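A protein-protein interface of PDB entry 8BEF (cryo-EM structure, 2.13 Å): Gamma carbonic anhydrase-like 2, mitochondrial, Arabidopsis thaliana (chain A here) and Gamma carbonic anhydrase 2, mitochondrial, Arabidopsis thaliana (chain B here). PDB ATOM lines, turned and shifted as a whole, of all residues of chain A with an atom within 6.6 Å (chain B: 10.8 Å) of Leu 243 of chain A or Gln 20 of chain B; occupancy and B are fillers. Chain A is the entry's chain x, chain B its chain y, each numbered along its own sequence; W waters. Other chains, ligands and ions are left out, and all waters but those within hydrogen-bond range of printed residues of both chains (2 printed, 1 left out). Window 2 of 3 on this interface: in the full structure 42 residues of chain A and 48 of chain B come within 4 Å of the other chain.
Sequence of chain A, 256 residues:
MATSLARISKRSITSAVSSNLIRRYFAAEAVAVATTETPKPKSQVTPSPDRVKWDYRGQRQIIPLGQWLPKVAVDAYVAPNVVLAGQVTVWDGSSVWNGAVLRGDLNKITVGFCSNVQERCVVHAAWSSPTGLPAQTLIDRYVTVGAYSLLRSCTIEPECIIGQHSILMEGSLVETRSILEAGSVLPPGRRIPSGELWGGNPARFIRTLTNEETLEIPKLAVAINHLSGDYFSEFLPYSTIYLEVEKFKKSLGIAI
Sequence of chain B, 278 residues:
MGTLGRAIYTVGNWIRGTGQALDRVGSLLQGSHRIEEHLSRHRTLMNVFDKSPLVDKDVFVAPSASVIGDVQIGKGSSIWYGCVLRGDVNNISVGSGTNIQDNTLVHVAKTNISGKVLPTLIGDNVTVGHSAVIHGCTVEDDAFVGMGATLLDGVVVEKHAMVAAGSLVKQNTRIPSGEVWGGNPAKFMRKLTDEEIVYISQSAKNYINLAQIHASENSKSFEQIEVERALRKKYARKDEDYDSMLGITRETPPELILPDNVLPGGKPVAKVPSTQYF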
ATOM      1  N   SER A 239     -27.919  -4.693  25.452  1.00  0.00           N
ATOM      2  CA  SER A 239     -27.087  -4.783  26.638  1.00  0.00           C
ATOM      3  C   SER A 239     -25.620  -4.939  26.238  1.00  0.00           C
ATOM      4  O   SER A 239     -25.288  -5.208  25.084  1.00  0.00           O
ATOM      5  CB  SER A 239     -27.530  -5.955  27.512  1.00  0.00           C
ATOM      6  OG  SER A 239     -26.918  -5.886  28.786  1.00  0.00           O
ATOM      7  N   THR A 240     -24.732  -4.767  27.216  1.00  0.00           N
ATOM      8  CA  THR A 240     -23.304  -4.970  27.013  1.00  0.00           C
ATOM      9  C   THR A 240     -22.810  -6.284  27.614  1.00  0.00           C
ATOM     10  O   THR A 240     -21.602  -6.449  27.812  1.00  0.00           O
ATOM     11  CB  THR A 240     -22.508  -3.792  27.584  1.00  0.00           C
ATOM     12  OG1 THR A 240     -22.992  -3.467  28.891  1.00  0.00           O
ATOM     13  CG2 THR A 240     -22.634  -2.578  26.683  1.00  0.00           C
ATOM     14  N   ILE A 241     -23.721  -7.219  27.903  1.00  0.00           N
ATOM     15  CA  ILE A 241     -23.328  -8.499  28.489  1.00  0.00           C
ATOM     16  C   ILE A 241     -22.456  -9.291  27.525  1.00  0.00           C
ATOM     17  O   ILE A 241     -21.531  -9.998  27.943  1.00  0.00           O
ATOM     18  CB  ILE A 241     -24.572  -9.309  28.900  1.00  0.00           C
ATOM     19  CG1 ILE A 241     -25.458  -8.481  29.812  1.00  0.00           C
ATOM     20  CG2 ILE A 241     -24.164 -10.577  29.624  1.00  0.00           C
ATOM     21  CD1 ILE A 241     -24.730  -8.026  30.999  1.00  0.00           C
ATOM     22  N   TYR A 242     -22.743  -9.194  26.225  1.00  0.00           N
ATOM     23  CA  TYR A 242     -21.988  -9.964  25.242  1.00  0.00           C
ATOM     24  C   TYR A 242     -20.493  -9.683  25.331  1.00  0.00           C
ATOM     25  O   TYR A 242     -19.684 -10.574  25.065  1.00  0.00           O
ATOM     26  CB  TYR A 242     -22.527  -9.693  23.835  1.00  0.00           C
ATOM     27  CG  TYR A 242     -22.201  -8.333  23.256  1.00  0.00           C
ATOM     28  CD1 TYR A 242     -23.025  -7.241  23.492  1.00  0.00           C
ATOM     29  CD2 TYR A 242     -21.086  -8.147  22.448  1.00  0.00           C
ATOM     30  CE1 TYR A 242     -22.740  -5.999  22.954  1.00  0.00           C
ATOM     31  CE2 TYR A 242     -20.793  -6.908  21.903  1.00  0.00           C
ATOM     32  CZ  TYR A 242     -21.624  -5.839  22.160  1.00  0.00           C
ATOM     33  OH  TYR A 242     -21.336  -4.604  21.624  1.00  0.00           O
ATOM     34  N   LEU A 243     -20.107  -8.470  25.733  1.00  0.00           N
ATOM     35  CA  LEU A 243     -18.697  -8.178  25.975  1.00  0.00           C
ATOM     36  C   LEU A 243     -18.142  -9.021  27.120  1.00  0.00           C
ATOM     37  O   LEU A 243     -17.018  -9.538  27.041  1.00  0.00           O
ATOM     38  CB  LEU A 243     -18.522  -6.693  26.281  1.00  0.00           C
ATOM     39  CG  LEU A 243     -18.603  -5.720  25.105  1.00  0.00           C
ATOM     40  CD1 LEU A 243     -17.977  -4.394  25.493  1.00  0.00           C
ATOM     41  CD2 LEU A 243     -17.919  -6.310  23.883  1.00  0.00           C
ATOM     42  N   GLU A 244     -18.912  -9.145  28.206  1.00  0.00           N
ATOM     43  CA  GLU A 244     -18.500  -9.980  29.328  1.00  0.00           C
ATOM     44  C   GLU A 244     -18.369 -11.432  28.902  1.00  0.00           C
ATOM     45  O   GLU A 244     -17.419 -12.121  29.292  1.00  0.00           O
ATOM     46  CB  GLU A 244     -19.506  -9.857  30.475  1.00  0.00           C
ATOM     47  CG  GLU A 244     -19.656  -8.495  31.191  1.00  0.00           C
ATOM     48  CD  GLU A 244     -18.378  -7.679  31.416  1.00  0.00           C
ATOM     49  OE1 GLU A 244     -17.262  -8.107  31.064  1.00  0.00           O
ATOM     50  OE2 GLU A 244     -18.503  -6.563  31.966  1.00  0.00           O
ATOM     51  N   VAL A 245     -19.322 -11.914  28.106  1.00  0.00           N
ATOM     52  CA  VAL A 245     -19.236 -13.265  27.563  1.00  0.00           C
ATOM     53  C   VAL A 245     -17.974 -13.421  26.722  1.00  0.00           C
ATOM     54  O   VAL A 245     -17.291 -14.447  26.788  1.00  0.00           O
ATOM     55  CB  VAL A 245     -20.503 -13.596  26.753  1.00  0.00           C
ATOM     56  CG1 VAL A 245     -20.495 -15.051  26.320  1.00  0.00           C
ATOM     57  CG2 VAL A 245     -21.749 -13.289  27.566  1.00  0.00           C
ATOM     58  N   GLU A 246     -17.644 -12.398  25.929  1.00  0.00           N
ATOM     59  CA  GLU A 246     -16.452 -12.448  25.087  1.00  0.00           C
ATOM     60  C   GLU A 246     -15.187 -12.603  25.923  1.00  0.00           C
ATOM     61  O   GLU A 246     -14.329 -13.441  25.623  1.00  0.00           O
ATOM     62  CB  GLU A 246     -16.357 -11.183  24.234  1.00  0.00           C
ATOM     63  CG  GLU A 246     -15.573 -11.353  22.954  1.00  0.00           C
ATOM     64  CD  GLU A 246     -15.464 -10.066  22.160  1.00  0.00           C
ATOM     65  OE1 GLU A 246     -16.275  -9.144  22.394  1.00  0.00           O
ATOM     66  OE2 GLU A 246     -14.564  -9.977  21.299  1.00  0.00           O
ATOM     67  N   LYS A 247     -15.045 -11.792  26.973  1.00  0.00           N
ATOM     68  CA  LYS A 247     -13.809 -11.878  27.752  1.00  0.00           C
ATOM     69  C   LYS A 247     -13.775 -13.146  28.602  1.00  0.00           C
ATOM     70  O   LYS A 247     -12.704 -13.725  28.816  1.00  0.00           O
ATOM     71  CB  LYS A 247     -13.604 -10.636  28.619  1.00  0.00           C
ATOM     72  CG  LYS A 247     -14.834 -10.017  29.204  1.00  0.00           C
ATOM     73  CD  LYS A 247     -14.437  -9.022  30.275  1.00  0.00           C
ATOM     74  CE  LYS A 247     -13.844  -7.760  29.667  1.00  0.00           C
ATOM     75  NZ  LYS A 247     -14.619  -7.286  28.487  1.00  0.00           N
ATOM     76  N   PHE A 248     -14.937 -13.596  29.087  1.00  0.00           N
ATOM     77  CA  PHE A 248     -15.010 -14.877  29.782  1.00  0.00           C
ATOM     78  C   PHE A 248     -14.564 -16.013  28.870  1.00  0.00           C
ATOM     79  O   PHE A 248     -13.902 -16.955  29.316  1.00  0.00           O
ATOM     80  CB  PHE A 248     -16.439 -15.108  30.280  1.00  0.00           C
ATOM     81  CG  PHE A 248     -16.560 -16.136  31.373  1.00  0.00           C
ATOM     82  CD1 PHE A 248     -16.600 -17.486  31.075  1.00  0.00           C
ATOM     83  CD2 PHE A 248     -16.663 -15.748  32.701  1.00  0.00           C
ATOM     84  CE1 PHE A 248     -16.723 -18.432  32.079  1.00  0.00           C
ATOM     85  CE2 PHE A 248     -16.786 -16.692  33.707  1.00  0.00           C
ATOM     86  CZ  PHE A 248     -16.815 -18.034  33.395  1.00  0.00           C
ATOM     87  N   GLY B  12     -12.363  -2.768  11.555  1.00  0.00           N
ATOM     88  CA  GLY B  12     -13.378  -3.123  12.533  1.00  0.00           C
ATOM     89  C   GLY B  12     -12.855  -3.068  13.955  1.00  0.00           C
ATOM     90  O   GLY B  12     -13.562  -2.644  14.869  1.00  0.00           O
ATOM     91  N   ASN B  13     -11.605  -3.486  14.157  1.00  0.00           N
ATOM     92  CA  ASN B  13     -10.985  -3.365  15.476  1.00  0.00           C
ATOM     93  C   ASN B  13     -10.920  -1.907  15.918  1.00  0.00           C
ATOM     94  O   ASN B  13     -11.240  -1.576  17.068  1.00  0.00           O
ATOM     95  CB  ASN B  13      -9.586  -3.980  15.455  1.00  0.00           C
ATOM     96  CG  ASN B  13      -9.560  -5.396  15.979  1.00  0.00           C
ATOM     97  OD1 ASN B  13     -10.570  -5.919  16.441  1.00  0.00           O
ATOM     98  ND2 ASN B  13      -8.400  -6.028  15.900  1.00  0.00           N
ATOM     99  N   TRP B  14     -10.505  -1.021  15.009  1.00  0.00           N
ATOM    100  CA  TRP B  14     -10.455   0.405  15.337  1.00  0.00           C
ATOM    101  C   TRP B  14     -11.837   0.941  15.700  1.00  0.00           C
ATOM    102  O   TRP B  14     -11.991   1.696  16.670  1.00  0.00           O
ATOM    103  CB  TRP B  14      -9.885   1.204  14.166  1.00  0.00           C
ATOM    104  CG  TRP B  14      -8.460   0.920  13.845  1.00  0.00           C
ATOM    105  CD1 TRP B  14      -7.557   0.257  14.619  1.00  0.00           C
ATOM    106  CD2 TRP B  14      -7.772   1.285  12.647  1.00  0.00           C
ATOM    107  NE1 TRP B  14      -6.345   0.193  13.979  1.00  0.00           N
ATOM    108  CE2 TRP B  14      -6.451   0.817  12.764  1.00  0.00           C
ATOM    109  CE3 TRP B  14      -8.145   1.967  11.484  1.00  0.00           C
ATOM    110  CZ2 TRP B  14      -5.503   1.005  11.766  1.00  0.00           C
ATOM    111  CZ3 TRP B  14      -7.205   2.152  10.497  1.00  0.00           C
ATOM    112  CH2 TRP B  14      -5.898   1.675  10.642  1.00  0.00           C
ATOM    113  N   ILE B  15     -12.850   0.568  14.916  1.00  0.00           N
ATOM    114  CA  ILE B  15     -14.208   1.041  15.167  1.00  0.00           C
ATOM    115  C   ILE B  15     -14.713   0.533  16.514  1.00  0.00           C
ATOM    116  O   ILE B  15     -15.385   1.258  17.254  1.00  0.00           O
ATOM    117  CB  ILE B  15     -15.138   0.630  14.009  1.00  0.00           C
ATOM    118  CG1 ILE B  15     -14.703   1.323  12.717  1.00  0.00           C
ATOM    119  CG2 ILE B  15     -16.588   0.965  14.330  1.00  0.00           C
ATOM    120  CD1 ILE B  15     -15.585   1.021  11.536  1.00  0.00           C
ATOM    121  N   ARG B  16     -14.389  -0.716  16.854  1.00  0.00           N
ATOM    122  CA  ARG B  16     -14.792  -1.263  18.148  1.00  0.00           C
ATOM    123  C   ARG B  16     -14.130  -0.516  19.298  1.00  0.00           C
ATOM    124  O   ARG B  16     -14.781  -0.203  20.305  1.00  0.00           O
ATOM    125  CB  ARG B  16     -14.449  -2.748  18.213  1.00  0.00           C
ATOM    126  CG  ARG B  16     -15.283  -3.612  17.296  1.00  0.00           C
ATOM    127  CD  ARG B  16     -15.244  -5.049  17.747  1.00  0.00           C
ATOM    128  NE  ARG B  16     -15.856  -5.197  19.059  1.00  0.00           N
ATOM    129  CZ  ARG B  16     -15.720  -6.261  19.835  1.00  0.00           C
ATOM    130  NH1 ARG B  16     -14.993  -7.300  19.460  1.00  0.00           N
ATOM    131  NH2 ARG B  16     -16.335  -6.286  21.012  1.00  0.00           N
ATOM    132  N   GLY B  17     -12.830  -0.239  19.176  1.00  0.00           N
ATOM    133  CA  GLY B  17     -12.158   0.539  20.205  1.00  0.00           C
ATOM    134  C   GLY B  17     -12.792   1.904  20.393  1.00  0.00           C
ATOM    135  O   GLY B  17     -13.053   2.334  21.521  1.00  0.00           O
ATOM    136  N   THR B  18     -13.081   2.588  19.281  1.00  0.00           N
ATOM    137  CA  THR B  18     -13.727   3.894  19.367  1.00  0.00           C
ATOM    138  C   THR B  18     -15.099   3.795  20.024  1.00  0.00           C
ATOM    139  O   THR B  18     -15.463   4.639  20.852  1.00  0.00           O
ATOM    140  CB  THR B  18     -13.852   4.520  17.976  1.00  0.00           C
ATOM    141  OG1 THR B  18     -12.564   4.573  17.352  1.00  0.00           O
ATOM    142  CG2 THR B  18     -14.427   5.924  18.075  1.00  0.00           C
ATOM    143  N   GLY B  19     -15.880   2.776  19.660  1.00  0.00           N
ATOM    144  CA  GLY B  19     -17.206   2.636  20.236  1.00  0.00           C
ATOM    145  C   GLY B  19     -17.174   2.395  21.733  1.00  0.00           C
ATOM    146  O   GLY B  19     -17.953   2.986  22.485  1.00  0.00           O
ATOM    147  N   GLN B  20     -16.269   1.526  22.187  1.00  0.00           N
ATOM    148  CA  GLN B  20     -16.168   1.281  23.622  1.00  0.00           C
ATOM    149  C   GLN B  20     -15.646   2.509  24.368  1.00  0.00           C
ATOM    150  O   GLN B  20     -16.080   2.779  25.498  1.00  0.00           O
ATOM    151  CB  GLN B  20     -15.303   0.046  23.877  1.00  0.00           C
ATOM    152  CG  GLN B  20     -15.873  -1.210  23.215  1.00  0.00           C
ATOM    153  CD  GLN B  20     -15.235  -2.496  23.696  1.00  0.00           C
ATOM    154  OE1 GLN B  20     -14.879  -2.631  24.865  1.00  0.00           O
ATOM    155  NE2 GLN B  20     -15.100  -3.459  22.792  1.00  0.00           N
ATOM    156  N   ALA B  21     -14.755   3.289  23.747  1.00  0.00           N
ATOM    157  CA  ALA B  21     -14.334   4.546  24.363  1.00  0.00           C
ATOM    158  C   ALA B  21     -15.503   5.518  24.498  1.00  0.00           C
ATOM    159  O   ALA B  21     -15.655   6.179  25.533  1.00  0.00           O
ATOM    160  CB  ALA B  21     -13.200   5.176  23.556  1.00  0.00           C
ATOM    161  N   LEU B  22     -16.336   5.620  23.460  1.00  0.00           N
ATOM    162  CA  LEU B  22     -17.511   6.483  23.537  1.00  0.00           C
ATOM    163  C   LEU B  22     -18.471   6.011  24.621  1.00  0.00           C
ATOM    164  O   LEU B  22     -19.073   6.828  25.326  1.00  0.00           O
ATOM    165  CB  LEU B  22     -18.222   6.541  22.185  1.00  0.00           C
ATOM    166  CG  LEU B  22     -17.674   7.534  21.159  1.00  0.00           C
ATOM    167  CD1 LEU B  22     -18.574   7.595  19.934  1.00  0.00           C
ATOM    168  CD2 LEU B  22     -17.529   8.909  21.780  1.00  0.00           C
ATOM    169  N   ASP B  23     -18.635   4.694  24.761  1.00  0.00           N
ATOM    170  CA  ASP B  23     -19.492   4.170  25.821  1.00  0.00           C
ATOM    171  C   ASP B  23     -18.950   4.541  27.198  1.00  0.00           C
ATOM    172  O   ASP B  23     -19.715   4.927  28.090  1.00  0.00           O
ATOM    173  CB  ASP B  23     -19.637   2.653  25.684  1.00  0.00           C
ATOM    174  CG  ASP B  23     -20.806   2.097  26.485  1.00  0.00           C
ATOM    175  OD1 ASP B  23     -21.795   2.824  26.698  1.00  0.00           O
ATOM    176  OD2 ASP B  23     -20.736   0.924  26.904  1.00  0.00           O
ATOM    177  N   ARG B  24     -17.630   4.445  27.385  1.00  0.00           N
ATOM    178  CA  ARG B  24     -17.044   4.838  28.665  1.00  0.00           C
ATOM    179  C   ARG B  24     -17.243   6.327  28.938  1.00  0.00           C
ATOM    180  O   ARG B  24     -17.566   6.722  30.065  1.00  0.00           O
ATOM    181  CB  ARG B  24     -15.559   4.479  28.707  1.00  0.00           C
ATOM    182  CG  ARG B  24     -15.301   3.050  29.127  1.00  0.00           C
ATOM    183  CD  ARG B  24     -13.844   2.636  28.961  1.00  0.00           C
ATOM    184  NE  ARG B  24     -13.121   3.423  27.969  1.00  0.00           N
ATOM    185  CZ  ARG B  24     -12.462   2.905  26.942  1.00  0.00           C
ATOM    186  NH1 ARG B  24     -12.461   1.603  26.707  1.00  0.00           N
ATOM    187  NH2 ARG B  24     -11.778   3.712  26.136  1.00  0.00           N
ATOM    188  N   VAL B  25     -17.058   7.168  27.919  1.00  0.00           N
ATOM    189  CA  VAL B  25     -17.264   8.605  28.097  1.00  0.00           C
ATOM    190  C   VAL B  25     -18.714   8.894  28.475  1.00  0.00           C
ATOM    191  O   VAL B  25     -18.992   9.711  29.363  1.00  0.00           O
ATOM    192  CB  VAL B  25     -16.839   9.371  26.830  1.00  0.00           C
ATOM    193  CG1 VAL B  25     -17.285  10.820  26.913  1.00  0.00           C
ATOM    194  CG2 VAL B  25     -15.332   9.289  26.647  1.00  0.00           C
ATOM    195  N   GLY B  26     -19.659   8.225  27.810  1.00  0.00           N
ATOM    196  CA  GLY B  26     -21.060   8.411  28.149  1.00  0.00           C
ATOM    197  C   GLY B  26     -21.387   7.955  29.557  1.00  0.00           C
ATOM    198  O   GLY B  26     -22.199   8.575  30.249  1.00  0.00           O
ATOM    199  N   SER B  27     -20.766   6.861  30.000  1.00  0.00           N
ATOM    200  CA  SER B  27     -20.946   6.419  31.378  1.00  0.00           C
ATOM    201  C   SER B  27     -20.412   7.454  32.362  1.00  0.00           C
ATOM    202  O   SER B  27     -21.034   7.713  33.398  1.00  0.00           O
ATOM    203  CB  SER B  27     -20.262   5.071  31.593  1.00  0.00           C
ATOM    204  OG  SER B  27     -20.811   4.083  30.740  1.00  0.00           O
ATOM    205  N   LEU B  28     -19.257   8.049  32.056  1.00  0.00           N
ATOM    206  CA  LEU B  28     -18.723   9.105  32.913  1.00  0.00           C
ATOM    207  C   LEU B  28     -19.675  10.291  32.977  1.00  0.00           C
ATOM    208  O   LEU B  28     -19.904  10.854  34.053  1.00  0.00           O
ATOM    209  CB  LEU B  28     -17.344   9.546  32.420  1.00  0.00           C
ATOM    210  CG  LEU B  28     -16.230   8.522  32.636  1.00  0.00           C
ATOM    211  CD1 LEU B  28     -14.897   9.062  32.167  1.00  0.00           C
ATOM    212  CD2 LEU B  28     -16.166   8.137  34.105  1.00  0.00           C
ATOM    213  N   GLU B  36     -24.064  -1.426  36.246  1.00  0.00           N
ATOM    214  CA  GLU B  36     -23.882  -2.145  34.993  1.00  0.00           C
ATOM    215  C   GLU B  36     -24.502  -3.536  35.050  1.00  0.00           C
ATOM    216  O   GLU B  36     -24.426  -4.230  36.066  1.00  0.00           O
ATOM    217  CB  GLU B  36     -22.398  -2.259  34.651  1.00  0.00           C
ATOM    218  CG  GLU B  36     -21.729  -0.933  34.373  1.00  0.00           C
ATOM    219  CD  GLU B  36     -20.615  -1.054  33.352  1.00  0.00           C
ATOM    220  OE1 GLU B  36     -19.709  -1.888  33.557  1.00  0.00           O
ATOM    221  OE2 GLU B  36     -20.648  -0.320  32.342  1.00  0.00           O
ATOM    222  N   GLU B  37     -25.127  -3.929  33.946  1.00  0.00           N
ATOM    223  CA  GLU B  37     -25.556  -5.306  33.771  1.00  0.00           C
ATOM    224  C   GLU B  37     -24.335  -6.219  33.703  1.00  0.00           C
ATOM    225  O   GLU B  37     -23.269  -5.829  33.223  1.00  0.00           O
ATOM    226  CB  GLU B  37     -26.397  -5.423  32.499  1.00  0.00           C
ATOM    227  CG  GLU B  37     -27.635  -4.535  32.495  1.00  0.00           C
ATOM    228  CD  GLU B  37     -28.339  -4.531  31.160  1.00  0.00           C
ATOM    229  OE1 GLU B  37     -28.539  -3.439  30.595  1.00  0.00           O
ATOM    230  OE2 GLU B  37     -28.659  -5.625  30.656  1.00  0.00           O
ATOM    231  N   HIS B  38     -24.490  -7.446  34.193  1.00  0.00           N
ATOM    232  CA  HIS B  38     -23.363  -8.364  34.293  1.00  0.00           C
ATOM    233  C   HIS B  38     -23.788  -9.768  33.883  1.00  0.00           C
ATOM    234  O   HIS B  38     -24.965 -10.045  33.643  1.00  0.00           O
ATOM    235  CB  HIS B  38     -22.773  -8.377  35.707  1.00  0.00           C
ATOM    236  CG  HIS B  38     -22.205  -7.062  36.135  1.00  0.00           C
ATOM    237  ND1 HIS B  38     -21.232  -6.402  35.415  1.00  0.00           N
ATOM    238  CD2 HIS B  38     -22.471  -6.283  37.211  1.00  0.00           C
ATOM    239  CE1 HIS B  38     -20.928  -5.270  36.026  1.00  0.00           C
ATOM    240  NE2 HIS B  38     -21.663  -5.175  37.119  1.00  0.00           N
ATOM    241  N   LEU B  39     -22.798 -10.653  33.800  1.00  0.00           N
ATOM    242  CA  LEU B  39     -23.056 -12.061  33.532  1.00  0.00           C
ATOM    243  C   LEU B  39     -23.959 -12.646  34.610  1.00  0.00           C
ATOM    244  O   LEU B  39     -23.815 -12.340  35.795  1.00  0.00           O
ATOM    245  CB  LEU B  39     -21.737 -12.828  33.478  1.00  0.00           C
ATOM    246  CG  LEU B  39     -21.691 -14.084  32.614  1.00  0.00           C
ATOM    247  CD1 LEU B  39     -22.180 -13.790  31.209  1.00  0.00           C
ATOM    248  CD2 LEU B  39     -20.288 -14.649  32.598  1.00  0.00           C
ATOM    249  N   SER B  40     -24.896 -13.494  34.192  1.00  0.00           N
ATOM    250  CA  SER B  40     -25.867 -14.045  35.126  1.00  0.00           C
ATOM    251  C   SER B  40     -25.182 -14.952  36.140  1.00  0.00           C
ATOM    252  O   SER B  40     -24.433 -15.863  35.774  1.00  0.00           O
ATOM    253  CB  SER B  40     -26.954 -14.815  34.379  1.00  0.00           C
ATOM    254  OG  SER B  40     -27.888 -15.377  35.283  1.00  0.00           O
HETATM  255  O   HOH W   1     -25.866  -2.726  29.284  1.00  0.00           O
HETATM  256  O   HOH W   2     -23.224  -1.842  31.478  1.00  0.00           O
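OE1 of Glu 246 of chain A is in salt-bridge range of NH2 of Arg 16 of chain B. OG of Ser 239 of chain A sits at hydrogen-bond distance from OE2 of Glu 37 of chain B.
The backbone carbonyl oxygen (O) of Glu 36 of chain B lies close to a ring nitrogen (NE2) of His 38 of chain B (3.1 Å). The backbone carbonyl oxygen of Asp 23 of chain B lies within hydrogen-bond range of the side-chain hydroxyl of Ser 27 of chain B.
Among the printed residues, merely in contact across the chains: Thr 240 of chain A with Asp 23 of chain B (3.99 Å), Ile 241 of chain A with Glu 37 of chain B (3.3 Å), Ile 241 of chain A with His 38 of chain B (3.3 Å), Leu 243 of chain A with Arg 16 of chain B (3.3 Å), Leu 243 of chain A with Gln 20 of chain B (3.6 Å), Val 245 of chain A with Leu 39 of chain B (3.7 Å) and Phe 248 of chain A with Leu 39 of chain B (3.8 Å).
Leu 243 of chain A touches two residues of chain B. Tyr 242 of chain A touches none of the printed residues of chain B. No residue of chain B comes within 4 Å of Glu 244 of chain A. Val 245 of chain A touches just one residue of chain B: Leu 39. No residue of chain B comes within 4 Å of Lys 247 of chain A. Printed residues of chain A within 4 Å of Arg 16 of chain B: Leu 243 (3.3 Å) and Glu 246 (3.2 Å). Of the printed residues of chain B, Phe 248 of chain A touches Leu 39 (3.8 Å). The nearest residue of chain B that does not touch Leu 243 of chain A is Asp 23 of chain B (6.2 Å). The nearest printed residue of chain B that does not touch Ile 241 of chain A is Leu 39 of chain B (4.1 Å).
Of the 10 printed residues of chain A, 7 touch a printed residue of chain B. Hydrophobic or aromatic side chains of chain A within 4 Å of the printed part of chain B: Ile 241, Leu 243, Val 245 and Phe 248.
Water W1 lies within hydrogen-bond range of the side-chain hydroxyl (OG1) of Thr 240 of chain A (3.0 Å), the side-chain carboxylate (OE1) of Glu 37 of chain B (3.1 Å) and the side-chain hydroxyl (OG) of Ser 239 of chain A (3.4 Å). Water W2 lies within hydrogen-bond range of the side-chain hydroxyl (OG1) of Thr 240 of chain A (3.1 Å) and the side-chain carboxylate (OE2) of Glu 36 of chain B (3.1 Å).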
